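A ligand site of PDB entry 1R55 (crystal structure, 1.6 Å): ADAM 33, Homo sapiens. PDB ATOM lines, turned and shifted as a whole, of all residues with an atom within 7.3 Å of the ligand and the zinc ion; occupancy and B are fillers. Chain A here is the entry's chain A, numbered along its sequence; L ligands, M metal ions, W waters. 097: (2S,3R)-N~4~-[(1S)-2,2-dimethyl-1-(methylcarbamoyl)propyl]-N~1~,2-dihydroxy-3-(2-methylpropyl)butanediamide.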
ATOM      1  N   GLY A 105       7.900   2.341   7.971  1.00  0.00           N
ATOM      2  CA  GLY A 105       7.038   1.806   9.012  1.00  0.00           C
ATOM      3  C   GLY A 105       5.585   1.588   8.632  1.00  0.00           C
ATOM      4  O   GLY A 105       4.737   1.367   9.490  1.00  0.00           O
ATOM      5  N   ALA A 106       5.302   1.652   7.332  1.00  0.00           N
ATOM      6  CA  ALA A 106       3.944   1.457   6.815  1.00  0.00           C
ATOM      7  C   ALA A 106       2.961   2.536   7.284  1.00  0.00           C
ATOM      8  O   ALA A 106       1.756   2.404   7.112  1.00  0.00           O
ATOM      9  CB  ALA A 106       3.425   0.076   7.218  1.00  0.00           C
ATOM     10  N   THR A 107       3.483   3.609   7.873  1.00  0.00           N
ATOM     11  CA  THR A 107       2.644   4.692   8.337  1.00  0.00           C
ATOM     12  C   THR A 107       2.086   5.441   7.129  1.00  0.00           C
ATOM     13  O   THR A 107       2.836   5.770   6.210  1.00  0.00           O
ATOM     14  CB  THR A 107       3.430   5.680   9.205  1.00  0.00           C
ATOM     15  OG1 THR A 107       3.926   5.005  10.375  1.00  0.00           O
ATOM     16  CG2 THR A 107       2.551   6.841   9.642  1.00  0.00           C
ATOM     17  N   VAL A 108       0.787   5.713   7.140  1.00  0.00           N
ATOM     18  CA  VAL A 108       0.178   6.434   6.019  1.00  0.00           C
ATOM     19  C   VAL A 108      -0.283   7.844   6.386  1.00  0.00           C
ATOM     20  O   VAL A 108      -0.629   8.626   5.498  1.00  0.00           O
ATOM     21  CB  VAL A 108      -1.014   5.654   5.402  1.00  0.00           C
ATOM     22  CG1 VAL A 108      -0.503   4.422   4.679  1.00  0.00           C
ATOM     23  CG2 VAL A 108      -2.016   5.251   6.479  1.00  0.00           C
ATOM     24  N   GLY A 109      -0.278   8.173   7.674  1.00  0.00           N
ATOM     25  CA  GLY A 109      -0.687   9.494   8.097  1.00  0.00           C
ATOM     26  C   GLY A 109      -0.349   9.808   9.546  1.00  0.00           C
ATOM     27  O   GLY A 109      -0.213   8.894  10.363  1.00  0.00           O
ATOM     28  N   LEU A 110      -0.216  11.098   9.860  1.00  0.00           N
ATOM     29  CA  LEU A 110       0.113  11.564  11.209  1.00  0.00           C
ATOM     30  C   LEU A 110      -0.458  12.966  11.454  1.00  0.00           C
ATOM     31  O   LEU A 110      -0.640  13.737  10.525  1.00  0.00           O
ATOM     32  CB  LEU A 110       1.625  11.656  11.403  1.00  0.00           C
ATOM     33  CG  LEU A 110       2.321  10.333  11.709  1.00  0.00           C
ATOM     34  CD1 LEU A 110       3.833  10.556  11.831  1.00  0.00           C
ATOM     35  CD2 LEU A 110       1.780   9.702  12.982  1.00  0.00           C
ATOM     36  N   ALA A 111      -0.690  13.293  12.722  1.00  0.00           N
ATOM     37  CA  ALA A 111      -1.206  14.609  13.103  1.00  0.00           C
ATOM     38  C   ALA A 111      -1.055  14.804  14.608  1.00  0.00           C
ATOM     39  O   ALA A 111      -1.159  13.862  15.381  1.00  0.00           O
ATOM     40  CB  ALA A 111      -2.677  14.728  12.714  1.00  0.00           C
ATOM     41  N   VAL A 125      -0.554  15.130   7.807  1.00  0.00           N
ATOM     42  CA  VAL A 125       0.018  14.638   6.555  1.00  0.00           C
ATOM     43  C   VAL A 125      -0.555  13.261   6.242  1.00  0.00           C
ATOM     44  O   VAL A 125      -0.778  12.462   7.157  1.00  0.00           O
ATOM     45  CB  VAL A 125       1.564  14.560   6.621  1.00  0.00           C
ATOM     46  CG1 VAL A 125       2.002  13.600   7.721  1.00  0.00           C
ATOM     47  CG2 VAL A 125       2.120  14.102   5.276  1.00  0.00           C
ATOM     48  N   SER A 126      -0.793  12.991   4.971  1.00  0.00           N
ATOM     49  CA  SER A 126      -1.353  11.718   4.529  1.00  0.00           C
ATOM     50  C   SER A 126      -0.738  11.303   3.199  1.00  0.00           C
ATOM     51  O   SER A 126      -0.523  12.135   2.326  1.00  0.00           O
ATOM     52  CB  SER A 126      -2.872  11.846   4.322  1.00  0.00           C
ATOM     53  OG  SER A 126      -3.542  12.297   5.477  1.00  0.00           O
ATOM     54  N   HIS A 129      -2.133   6.671  -0.740  1.00  0.00           N
ATOM     55  CA  HIS A 129      -1.818   5.247  -0.856  1.00  0.00           C
ATOM     56  C   HIS A 129      -2.725   4.332  -1.668  1.00  0.00           C
ATOM     57  O   HIS A 129      -2.324   3.216  -2.011  1.00  0.00           O
ATOM     58  CB  HIS A 129      -1.660   4.683   0.550  1.00  0.00           C
ATOM     59  CG  HIS A 129      -2.866   4.871   1.423  1.00  0.00           C
ATOM     60  ND1 HIS A 129      -3.963   4.043   1.377  1.00  0.00           N
ATOM     61  CD2 HIS A 129      -3.131   5.806   2.372  1.00  0.00           C
ATOM     62  CE1 HIS A 129      -4.860   4.453   2.256  1.00  0.00           C
ATOM     63  NE2 HIS A 129      -4.375   5.515   2.879  1.00  0.00           N
ATOM     64  N   GLY A 135      -9.479   6.366  -0.011  1.00  0.00           N
ATOM     65  CA  GLY A 135      -8.397   5.853   0.817  1.00  0.00           C
ATOM     66  C   GLY A 135      -7.685   6.997   1.519  1.00  0.00           C
ATOM     67  O   GLY A 135      -7.600   7.038   2.748  1.00  0.00           O
ATOM     68  N   ALA A 136      -7.181   7.928   0.726  1.00  0.00           N
ATOM     69  CA  ALA A 136      -6.486   9.104   1.254  1.00  0.00           C
ATOM     70  C   ALA A 136      -7.416   9.927   2.139  1.00  0.00           C
ATOM     71  O   ALA A 136      -6.997  10.471   3.158  1.00  0.00           O
ATOM     72  CB  ALA A 136      -5.975   9.959   0.110  1.00  0.00           C
ATOM     73  N   ALA A 138      -9.976   8.884   3.980  1.00  0.00           N
ATOM     74  CA  ALA A 138     -10.185   8.259   5.275  1.00  0.00           C
ATOM     75  C   ALA A 138      -8.978   8.498   6.168  1.00  0.00           C
ATOM     76  O   ALA A 138      -9.125   8.658   7.383  1.00  0.00           O
ATOM     77  CB  ALA A 138     -10.433   6.767   5.096  1.00  0.00           C
ATOM     78  N   THR A 139      -7.788   8.521   5.579  1.00  0.00           N
ATOM     79  CA  THR A 139      -6.580   8.770   6.344  1.00  0.00           C
ATOM     80  C   THR A 139      -6.584  10.224   6.813  1.00  0.00           C
ATOM     81  O   THR A 139      -6.328  10.520   7.970  1.00  0.00           O
ATOM     82  CB  THR A 139      -5.318   8.495   5.489  1.00  0.00           C
ATOM     83  OG1 THR A 139      -5.209   7.091   5.241  1.00  0.00           O
ATOM     84  CG2 THR A 139      -4.056   8.976   6.204  1.00  0.00           C
ATOM     85  N   MET A 140      -6.905  11.134   5.897  1.00  0.00           N
ATOM     86  CA  MET A 140      -6.939  12.553   6.228  1.00  0.00           C
ATOM     87  C   MET A 140      -7.984  12.841   7.305  1.00  0.00           C
ATOM     88  O   MET A 140      -7.748  13.642   8.209  1.00  0.00           O
ATOM     89  CB  MET A 140      -7.226  13.389   4.981  1.00  0.00           C
ATOM     90  CG  MET A 140      -6.997  14.880   5.171  1.00  0.00           C
ATOM     91  SD  MET A 140      -7.172  15.804   3.640  1.00  0.00           S
ATOM     92  CE  MET A 140      -5.715  15.309   2.766  1.00  0.00           C
ATOM     93  N   HIS A 142      -8.943  10.796   9.527  1.00  0.00           N
ATOM     94  CA  HIS A 142      -8.406  10.177  10.734  1.00  0.00           C
ATOM     95  C   HIS A 142      -7.454  11.170  11.409  1.00  0.00           C
ATOM     96  O   HIS A 142      -7.514  11.360  12.632  1.00  0.00           O
ATOM     97  CB  HIS A 142      -7.637   8.899  10.367  1.00  0.00           C
ATOM     98  CG  HIS A 142      -7.002   8.197  11.533  1.00  0.00           C
ATOM     99  ND1 HIS A 142      -7.572   7.109  12.154  1.00  0.00           N
ATOM    100  CD2 HIS A 142      -5.835   8.429  12.169  1.00  0.00           C
ATOM    101  CE1 HIS A 142      -6.775   6.686  13.114  1.00  0.00           C
ATOM    102  NE2 HIS A 142      -5.707   7.471  13.152  1.00  0.00           N
ATOM    103  N   GLU A 143      -6.594  11.807  10.623  1.00  0.00           N
ATOM    104  CA  GLU A 143      -5.660  12.776  11.189  1.00  0.00           C
ATOM    105  C   GLU A 143      -6.394  14.011  11.707  1.00  0.00           C
ATOM    106  O   GLU A 143      -6.015  14.595  12.731  1.00  0.00           O
ATOM    107  CB  GLU A 143      -4.599  13.184  10.158  1.00  0.00           C
ATOM    108  CG  GLU A 143      -3.846  12.036   9.494  1.00  0.00           C
ATOM    109  CD  GLU A 143      -3.471  10.899  10.443  1.00  0.00           C
ATOM    110  OE1 GLU A 143      -3.223  11.140  11.635  1.00  0.00           O
ATOM    111  OE2 GLU A 143      -3.415   9.742   9.966  1.00  0.00           O
ATOM    112  N   HIS A 146      -7.669  13.222  15.134  1.00  0.00           N
ATOM    113  CA  HIS A 146      -6.700  13.396  16.201  1.00  0.00           C
ATOM    114  C   HIS A 146      -6.602  14.875  16.564  1.00  0.00           C
ATOM    115  O   HIS A 146      -6.493  15.225  17.732  1.00  0.00           O
ATOM    116  CB  HIS A 146      -5.309  12.902  15.789  1.00  0.00           C
ATOM    117  CG  HIS A 146      -5.146  11.408  15.842  1.00  0.00           C
ATOM    118  ND1 HIS A 146      -5.429  10.674  16.973  1.00  0.00           N
ATOM    119  CD2 HIS A 146      -4.718  10.529  14.916  1.00  0.00           C
ATOM    120  CE1 HIS A 146      -5.166   9.394  16.737  1.00  0.00           C
ATOM    121  NE2 HIS A 146      -4.734   9.284  15.494  1.00  0.00           N
ATOM    122  N   LEU A 150      -9.703  13.231  19.105  1.00  0.00           N
ATOM    123  CA  LEU A 150     -10.259  11.890  19.031  1.00  0.00           C
ATOM    124  C   LEU A 150      -9.153  10.862  19.136  1.00  0.00           C
ATOM    125  O   LEU A 150      -8.086  11.016  18.550  1.00  0.00           O
ATOM    126  CB  LEU A 150     -11.010  11.686  17.700  1.00  0.00           C
ATOM    127  CG  LEU A 150     -12.058  12.771  17.436  1.00  0.00           C
ATOM    128  CD1 LEU A 150     -12.868  12.430  16.189  1.00  0.00           C
ATOM    129  CD2 LEU A 150     -12.998  12.947  18.628  1.00  0.00           C
ATOM    130  N   SER A 151      -9.394   9.801  19.900  1.00  0.00           N
ATOM    131  CA  SER A 151      -8.404   8.756  20.062  1.00  0.00           C
ATOM    132  C   SER A 151      -8.769   7.599  19.137  1.00  0.00           C
ATOM    133  O   SER A 151      -9.815   7.622  18.494  1.00  0.00           O
ATOM    134  CB  SER A 151      -8.381   8.256  21.508  1.00  0.00           C
ATOM    135  OG  SER A 151      -9.550   7.516  21.782  1.00  0.00           O
ATOM    136  N   HIS A 152      -7.896   6.604  19.057  1.00  0.00           N
ATOM    137  CA  HIS A 152      -8.195   5.448  18.233  1.00  0.00           C
ATOM    138  C   HIS A 152      -9.355   4.722  18.912  1.00  0.00           C
ATOM    139  O   HIS A 152      -9.450   4.710  20.152  1.00  0.00           O
ATOM    140  CB  HIS A 152      -6.979   4.533  18.128  1.00  0.00           C
ATOM    141  CG  HIS A 152      -5.912   5.048  17.218  1.00  0.00           C
ATOM    142  ND1 HIS A 152      -4.666   4.449  17.097  1.00  0.00           N
ATOM    143  CD2 HIS A 152      -5.891   6.112  16.376  1.00  0.00           C
ATOM    144  CE1 HIS A 152      -3.945   5.107  16.221  1.00  0.00           C
ATOM    145  NE2 HIS A 152      -4.659   6.124  15.761  1.00  0.00           N
ATOM    146  N   VAL A 169     -13.707   5.488  11.027  1.00  0.00           N
ATOM    147  CA  VAL A 169     -12.531   6.300  10.744  1.00  0.00           C
ATOM    148  C   VAL A 169     -11.398   6.252  11.765  1.00  0.00           C
ATOM    149  O   VAL A 169     -10.231   6.246  11.386  1.00  0.00           O
ATOM    150  CB  VAL A 169     -12.944   7.778  10.501  1.00  0.00           C
ATOM    151  CG1 VAL A 169     -11.713   8.641  10.259  1.00  0.00           C
ATOM    152  CG2 VAL A 169     -13.884   7.856   9.307  1.00  0.00           C
ATOM    153  N   MET A 170     -11.716   6.224  13.056  1.00  0.00           N
ATOM    154  CA  MET A 170     -10.644   6.196  14.045  1.00  0.00           C
ATOM    155  C   MET A 170     -10.018   4.837  14.356  1.00  0.00           C
ATOM    156  O   MET A 170      -9.418   4.650  15.419  1.00  0.00           O
ATOM    157  CB  MET A 170     -11.092   6.886  15.343  1.00  0.00           C
ATOM    158  CG  MET A 170     -11.337   8.397  15.189  1.00  0.00           C
ATOM    159  SD  MET A 170     -10.094   9.310  14.217  1.00  0.00           S
ATOM    160  CE  MET A 170      -8.617   9.100  15.217  1.00  0.00           C
ATOM    161  N   ALA A 171     -10.149   3.889  13.434  1.00  0.00           N
ATOM    162  CA  ALA A 171      -9.524   2.587  13.633  1.00  0.00           C
ATOM    163  C   ALA A 171      -8.023   2.854  13.542  1.00  0.00           C
ATOM    164  O   ALA A 171      -7.603   3.787  12.859  1.00  0.00           O
ATOM    165  CB  ALA A 171      -9.967   1.623  12.547  1.00  0.00           C
ATOM    166  N   ALA A 172      -7.218   2.023  14.208  1.00  0.00           N
ATOM    167  CA  ALA A 172      -5.771   2.197  14.213  1.00  0.00           C
ATOM    168  C   ALA A 172      -5.076   1.756  12.926  1.00  0.00           C
ATOM    169  O   ALA A 172      -3.947   2.160  12.650  1.00  0.00           O
ATOM    170  CB  ALA A 172      -5.171   1.436  15.395  1.00  0.00           C
ATOM    171  N   ALA A 173      -5.766   0.941  12.143  1.00  0.00           N
ATOM    172  CA  ALA A 173      -5.235   0.444  10.892  1.00  0.00           C
ATOM    173  C   ALA A 173      -6.228   0.736   9.782  1.00  0.00           C
ATOM    174  O   ALA A 173      -7.432   0.811  10.024  1.00  0.00           O
ATOM    175  CB  ALA A 173      -4.985  -1.058  10.985  1.00  0.00           C
ATOM    176  N   THR A 174      -5.720   0.906   8.563  1.00  0.00           N
ATOM    177  CA  THR A 174      -6.614   1.188   7.451  1.00  0.00           C
ATOM    178  C   THR A 174      -6.376   0.247   6.284  1.00  0.00           C
ATOM    179  O   THR A 174      -5.363  -0.453   6.213  1.00  0.00           O
ATOM    180  CB  THR A 174      -6.467   2.649   6.974  1.00  0.00           C
ATOM    181  OG1 THR A 174      -7.572   2.980   6.123  1.00  0.00           O
ATOM    182  CG2 THR A 174      -5.177   2.839   6.197  1.00  0.00           C
ATOM    183  N   GLY A 175      -7.329   0.247   5.361  1.00  0.00           N
ATOM    184  CA  GLY A 175      -7.239  -0.608   4.196  1.00  0.00           C
ATOM    185  C   GLY A 175      -8.633  -0.775   3.621  1.00  0.00           C
ATOM    186  O   GLY A 175      -9.623  -0.525   4.309  1.00  0.00           O
HETATM  187  N1  097 L   1      -1.664   2.802  10.254  1.00  0.00           N
HETATM  188  C2  097 L   1      -5.167   4.291  10.371  1.00  0.00           C
HETATM  189  O2  097 L   1      -2.800   0.789   8.556  1.00  0.00           O
HETATM  190  C4  097 L   1      -1.443   4.120  10.073  1.00  0.00           C
HETATM  191  O3  097 L   1      -2.873   8.854  13.187  1.00  0.00           O
HETATM  192  C5  097 L   1      -0.863   1.885   9.451  1.00  0.00           C
HETATM  193  C6  097 L   1      -0.251   0.804  10.354  1.00  0.00           C
HETATM  194  C8  097 L   1      -1.372   0.089  11.128  1.00  0.00           C
HETATM  195  C9  097 L   1       0.536  -0.205   9.506  1.00  0.00           C
HETATM  196  C10 097 L   1      -1.677   1.261   8.336  1.00  0.00           C
HETATM  197  C11 097 L   1      -1.752   0.653   6.002  1.00  0.00           C
HETATM  198  N3  097 L   1      -1.998   8.121  12.424  1.00  0.00           N
HETATM  199  C12 097 L   1      -2.097   6.817  12.720  1.00  0.00           C
HETATM  200  O4  097 L   1      -2.780   6.406  13.651  1.00  0.00           O
HETATM  201  C13 097 L   1      -1.348   5.861  11.829  1.00  0.00           C
HETATM  202  O5  097 L   1      -0.455   5.063  12.584  1.00  0.00           O
HETATM  203  C14 097 L   1      -2.285   5.007  10.980  1.00  0.00           C
HETATM  204  C15 097 L   1      -3.218   5.884  10.138  1.00  0.00           C
HETATM  205  C1  097 L   1      -4.326   5.112   9.400  1.00  0.00           C
HETATM  206  C3  097 L   1      -5.225   6.077   8.638  1.00  0.00           C
HETATM  207  O1  097 L   1      -0.655   4.597   9.271  1.00  0.00           O
HETATM  208  C7  097 L   1       0.704   1.489  11.354  1.00  0.00           C
HETATM  209  N2  097 L   1      -1.076   1.294   7.132  1.00  0.00           N
HETATM  210 ZN    ZN M   1      -4.011   7.665  14.472  1.00  0.00          ZN
HETATM  211  O   HOH W   1      -1.728   3.196  14.131  1.00  0.00           O
HETATM  212  O   HOH W   2      -2.914  -2.402   7.951  1.00  0.00           O
HETATM  213  O   HOH W   3      -1.109  10.539  14.432  1.00  0.00           O
HETATM  214  O   HOH W   4      -2.193   7.870  15.954  1.00  0.00           O
HETATM  215  O   HOH W   5       2.324   4.946  12.604  1.00  0.00           O
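The side-chain carboxylate (OE2) of Glu 143 sits at hydrogen-bond distance from a nitrogen (N3) of the ligand (3.3 Å).
The backbone NH (N) of Val 108 lies within hydrogen-bond range of an oxygen (O1) of the ligand (2.8 Å).
A nitrogen (N3) of the ligand sits at hydrogen-bond distance from the backbone carbonyl oxygen (O) of Gly 109, 2.8 Å away.
The backbone NH (N) of Thr 174 lies within hydrogen-bond range of an oxygen (O2) of the ligand.
The backbone carbonyl oxygen (O) of Ala 106 is in hydrogen-bond range of a nitrogen (N2) of the ligand, 3.0 Å away.
A nitrogen (N1) of the ligand lies close to the backbone carbonyl oxygen (O) of Ala 172, 3.4 Å away.
A ring nitrogen (ND1) of His 146 lies within hydrogen-bond range of the backbone carbonyl oxygen (O) of Leu 150, 3.1 Å away.
ND1 of His 142 lies close to O of Ala 171.
ND1 of His 142 lies within hydrogen-bond range of O of Val 169 (2.9 Å).
The backbone NH of Leu 110 sits close to the side-chain carboxylate of Glu 143 (3.5 Å).
The side-chain carboxylate (OE1) of Glu 143 is in hydrogen-bond range of the backbone NH (N) of Ala 111 (3.5 Å).
NE2 of His 129 sits at hydrogen-bond distance from OG1 of Thr 139 (3.0 Å).
O of Gly 135 is in hydrogen-bond range of OG1 of Thr 139, 3.5 Å away.
Thr 107 touches the ligand.
Thr 139 touches the ligand (OG1 to C3, 3.5 Å).
Ala 171 touches the ligand.
Ala 173 touches the ligand.
Hydrophobic or aromatic side chains that line the ligand: Ala 106, Val 108, His 142, His 146, His 152 and Ala 173.
Of the 28 residues printed, 13 come within 4 Å of the ligand.
Of the 28 residues printed, 3 come within 4 Å of the zinc ion.
The zinc ion is bound by an oxygen (O4) of the ligand (1.9 Å), a ring nitrogen (NE2) of His 146 (2.0 Å), an oxygen (O3) of the ligand (2.1 Å), a ring nitrogen (NE2) of His 152 (2.1 Å), a ring nitrogen (NE2) of His 142 (2.2 Å) and water W4 (2.4 Å).
The zinc ion has six donor atoms within binding distance.
Water W1 lies within hydrogen-bond range of an oxygen (O5) of the ligand (2.7 Å) and the backbone carbonyl oxygen (O) of Ala 172 (2.9 Å).
Water W3 bridges N3 of the ligand and N of Ala 111.
Water W5 bridges OG1 of Thr 107 (2.7 Å) and O5 of the ligand (2.8 Å).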
